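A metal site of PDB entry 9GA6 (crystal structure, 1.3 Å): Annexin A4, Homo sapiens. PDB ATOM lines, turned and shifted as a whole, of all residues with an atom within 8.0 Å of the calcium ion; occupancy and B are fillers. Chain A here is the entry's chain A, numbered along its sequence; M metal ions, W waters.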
ATOM      1  N   TYR A 255      32.063  25.926  17.521  1.00  0.00           N
ATOM      2  CA  TYR A 255      31.764  26.785  18.659  1.00  0.00           C
ATOM      3  C   TYR A 255      30.905  27.975  18.242  1.00  0.00           C
ATOM      4  O   TYR A 255      29.840  28.211  18.852  1.00  0.00           O
ATOM      5  CB  TYR A 255      33.092  27.220  19.273  1.00  0.00           C
ATOM      6  CG  TYR A 255      32.951  28.193  20.422  1.00  0.00           C
ATOM      7  CD1 TYR A 255      32.589  27.766  21.688  1.00  0.00           C
ATOM      8  CD2 TYR A 255      33.107  29.546  20.221  1.00  0.00           C
ATOM      9  CE1 TYR A 255      32.464  28.642  22.764  1.00  0.00           C
ATOM     10  CE2 TYR A 255      32.970  30.439  21.288  1.00  0.00           C
ATOM     11  CZ  TYR A 255      32.680  29.977  22.547  1.00  0.00           C
ATOM     12  OH  TYR A 255      32.527  30.834  23.637  1.00  0.00           O
ATOM     13  N   LYS A 256      31.343  28.642  17.192  1.00  0.00           N
ATOM     14  CA  LYS A 256      30.635  29.849  16.735  1.00  0.00           C
ATOM     15  C   LYS A 256      29.239  29.513  16.250  1.00  0.00           C
ATOM     16  O   LYS A 256      28.342  30.366  16.312  1.00  0.00           O
ATOM     17  CB  LYS A 256      31.498  30.627  15.743  1.00  0.00           C
ATOM     18  CG  LYS A 256      32.707  31.261  16.344  1.00  0.00           C
ATOM     19  CD  LYS A 256      33.509  32.100  15.358  1.00  0.00           C
ATOM     20  CE  LYS A 256      34.593  32.782  16.108  1.00  0.00           C
ATOM     21  NZ  LYS A 256      35.355  33.585  15.145  1.00  0.00           N
ATOM     22  N   SER A 257      29.040  28.325  15.662  1.00  0.00           N
ATOM     23  CA  SER A 257      27.732  27.968  15.152  1.00  0.00           C
ATOM     24  C   SER A 257      26.705  27.788  16.256  1.00  0.00           C
ATOM     25  O   SER A 257      25.517  27.796  15.966  1.00  0.00           O
ATOM     26  CB  SER A 257      27.795  26.712  14.301  1.00  0.00           C
ATOM     27  OG  SER A 257      27.946  25.491  15.046  1.00  0.00           O
ATOM     28  N   MET A 258      27.178  27.477  17.473  1.00  0.00           N
ATOM     29  CA  MET A 258      26.273  27.106  18.567  1.00  0.00           C
ATOM     30  C   MET A 258      26.288  28.116  19.730  1.00  0.00           C
ATOM     31  O   MET A 258      25.300  28.161  20.464  1.00  0.00           O
ATOM     32  CB  MET A 258      26.579  25.702  19.104  1.00  0.00           C
ATOM     33  CG  MET A 258      26.192  24.603  18.133  1.00  0.00           C
ATOM     34  SD  MET A 258      26.649  22.961  18.703  1.00  0.00           S
ATOM     35  CE  MET A 258      28.389  22.970  18.240  1.00  0.00           C
ATOM     36  N   LYS A 259      27.334  28.872  19.953  1.00  0.00           N
ATOM     37  CA  LYS A 259      27.429  29.711  21.161  1.00  0.00           C
ATOM     38  C   LYS A 259      26.386  30.811  21.069  1.00  0.00           C
ATOM     39  O   LYS A 259      26.027  31.268  20.003  1.00  0.00           O
ATOM     40  CB  LYS A 259      28.871  30.215  21.236  1.00  0.00           C
ATOM     41  CG  LYS A 259      29.207  31.061  22.477  1.00  0.00           C
ATOM     42  CD  LYS A 259      28.939  30.214  23.721  1.00  0.00           C
ATOM     43  CE  LYS A 259      29.556  30.741  24.978  1.00  0.00           C
ATOM     44  NZ  LYS A 259      30.047  29.581  25.710  1.00  0.00           N
ATOM     45  N   GLY A 260      25.825  31.218  22.209  1.00  0.00           N
ATOM     46  CA  GLY A 260      24.761  32.228  22.148  1.00  0.00           C
ATOM     47  C   GLY A 260      23.525  31.871  21.282  1.00  0.00           C
ATOM     48  O   GLY A 260      23.276  30.729  20.929  1.00  0.00           O
ATOM     49  N   LEU A 261      22.699  32.891  20.978  1.00  0.00           N
ATOM     50  CA  LEU A 261      21.284  32.674  20.759  1.00  0.00           C
ATOM     51  C   LEU A 261      21.045  31.902  19.466  1.00  0.00           C
ATOM     52  O   LEU A 261      21.437  32.326  18.401  1.00  0.00           O
ATOM     53  CB  LEU A 261      20.507  34.001  20.833  1.00  0.00           C
ATOM     54  CG  LEU A 261      20.785  35.087  19.766  1.00  0.00           C
ATOM     55  CD1 LEU A 261      19.816  35.035  18.588  1.00  0.00           C
ATOM     56  CD2 LEU A 261      20.732  36.505  20.368  1.00  0.00           C
ATOM     57  N   GLY A 262      20.364  30.764  19.559  1.00  0.00           N
ATOM     58  CA  GLY A 262      20.018  30.021  18.360  1.00  0.00           C
ATOM     59  C   GLY A 262      21.217  29.280  17.785  1.00  0.00           C
ATOM     60  O   GLY A 262      22.182  28.957  18.506  1.00  0.00           O
ATOM     61  N   THR A 263      21.142  28.918  16.502  1.00  0.00           N
ATOM     62  CA  THR A 263      22.118  27.983  15.971  1.00  0.00           C
ATOM     63  C   THR A 263      22.275  28.252  14.485  1.00  0.00           C
ATOM     64  O   THR A 263      21.275  28.314  13.757  1.00  0.00           O
ATOM     65  CB  THR A 263      21.674  26.533  16.170  1.00  0.00           C
ATOM     66  OG1 THR A 263      21.441  26.245  17.550  1.00  0.00           O
ATOM     67  CG2 THR A 263      22.736  25.580  15.667  1.00  0.00           C
ATOM     68  N   ASP A 264      23.525  28.294  14.009  1.00  0.00           N
ATOM     69  CA  ASP A 264      23.784  28.283  12.588  1.00  0.00           C
ATOM     70  C   ASP A 264      23.774  26.828  12.099  1.00  0.00           C
ATOM     71  O   ASP A 264      24.820  26.169  11.994  1.00  0.00           O
ATOM     72  CB  ASP A 264      25.092  28.971  12.284  1.00  0.00           C
ATOM     73  CG  ASP A 264      25.489  29.005  10.824  1.00  0.00           C
ATOM     74  OD1 ASP A 264      24.729  28.480   9.992  1.00  0.00           O
ATOM     75  OD2 ASP A 264      26.582  29.508  10.532  1.00  0.00           O
ATOM     76  N   PHE A 298      27.994  20.522  23.779  1.00  0.00           N
ATOM     77  CA  PHE A 298      27.495  21.676  23.056  1.00  0.00           C
ATOM     78  C   PHE A 298      26.370  21.222  22.146  1.00  0.00           C
ATOM     79  O   PHE A 298      25.310  21.832  22.066  1.00  0.00           O
ATOM     80  CB  PHE A 298      28.572  22.362  22.226  1.00  0.00           C
ATOM     81  CG  PHE A 298      29.120  23.629  22.823  1.00  0.00           C
ATOM     82  CD1 PHE A 298      29.737  23.614  24.055  1.00  0.00           C
ATOM     83  CD2 PHE A 298      29.088  24.839  22.142  1.00  0.00           C
ATOM     84  CE1 PHE A 298      30.224  24.755  24.607  1.00  0.00           C
ATOM     85  CE2 PHE A 298      29.612  25.995  22.707  1.00  0.00           C
ATOM     86  CZ  PHE A 298      30.184  25.924  23.953  1.00  0.00           C
ATOM     87  N   GLY A 301      23.201  20.305  24.018  1.00  0.00           N
ATOM     88  CA  GLY A 301      22.491  21.446  24.554  1.00  0.00           C
ATOM     89  C   GLY A 301      21.871  22.347  23.500  1.00  0.00           C
ATOM     90  O   GLY A 301      20.993  23.170  23.808  1.00  0.00           O
ATOM     91  N   ASP A 302      22.280  22.243  22.248  1.00  0.00           N
ATOM     92  CA  ASP A 302      21.854  23.196  21.243  1.00  0.00           C
ATOM     93  C   ASP A 302      20.867  22.600  20.242  1.00  0.00           C
ATOM     94  O   ASP A 302      20.389  23.357  19.375  1.00  0.00           O
ATOM     95  CB  ASP A 302      23.039  23.799  20.508  1.00  0.00           C
ATOM     96  CG  ASP A 302      23.072  25.331  20.496  1.00  0.00           C
ATOM     97  OD1 ASP A 302      23.171  25.880  21.619  1.00  0.00           O
ATOM     98  OD2 ASP A 302      23.116  25.941  19.402  1.00  0.00           O
ATOM     99  N   THR A 303      20.637  21.272  20.253  1.00  0.00           N
ATOM    100  CA  THR A 303      19.824  20.605  19.251  1.00  0.00           C
ATOM    101  C   THR A 303      18.910  19.631  19.974  1.00  0.00           C
ATOM    102  O   THR A 303      19.128  19.318  21.141  1.00  0.00           O
ATOM    103  CB  THR A 303      20.697  19.874  18.228  1.00  0.00           C
ATOM    104  OG1 THR A 303      21.435  18.796  18.816  1.00  0.00           O
ATOM    105  CG2 THR A 303      21.641  20.844  17.540  1.00  0.00           C
HETATM  106 CA    CA M   1      22.950  28.362  20.719  1.00  0.00          CA
HETATM  107  O   HOH W   1      22.937  28.522  23.083  1.00  0.00           O
HETATM  108  O   HOH W   2      20.368  28.440  21.076  1.00  0.00           O
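The calcium ion is bound by water W1 (2.4 Å), the backbone carbonyl oxygen (O) of Met 258 (2.4 Å), the backbone carbonyl oxygen (O) of Gly 260 (2.4 Å), the backbone carbonyl oxygen (O) of Gly 262 (2.4 Å), water W2 (2.6 Å), the side-chain carboxylate (OD1) of Asp 302 (2.6 Å) and the side-chain carboxylate (OD2) of Asp 302 (2.8 Å). The calcium ion has seven donor atoms within binding distance.
Four residues have an atom within 4 Å of the calcium ion: Met 258, Gly 260, Gly 262 and Asp 302. The nearest printed residue that does not touch the calcium ion is Thr 263 (4.1 Å).
The side-chain carboxylate (OD2) of Asp 302 lies close to the side-chain hydroxyl (OG1) of Thr 263 (2.5 Å).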
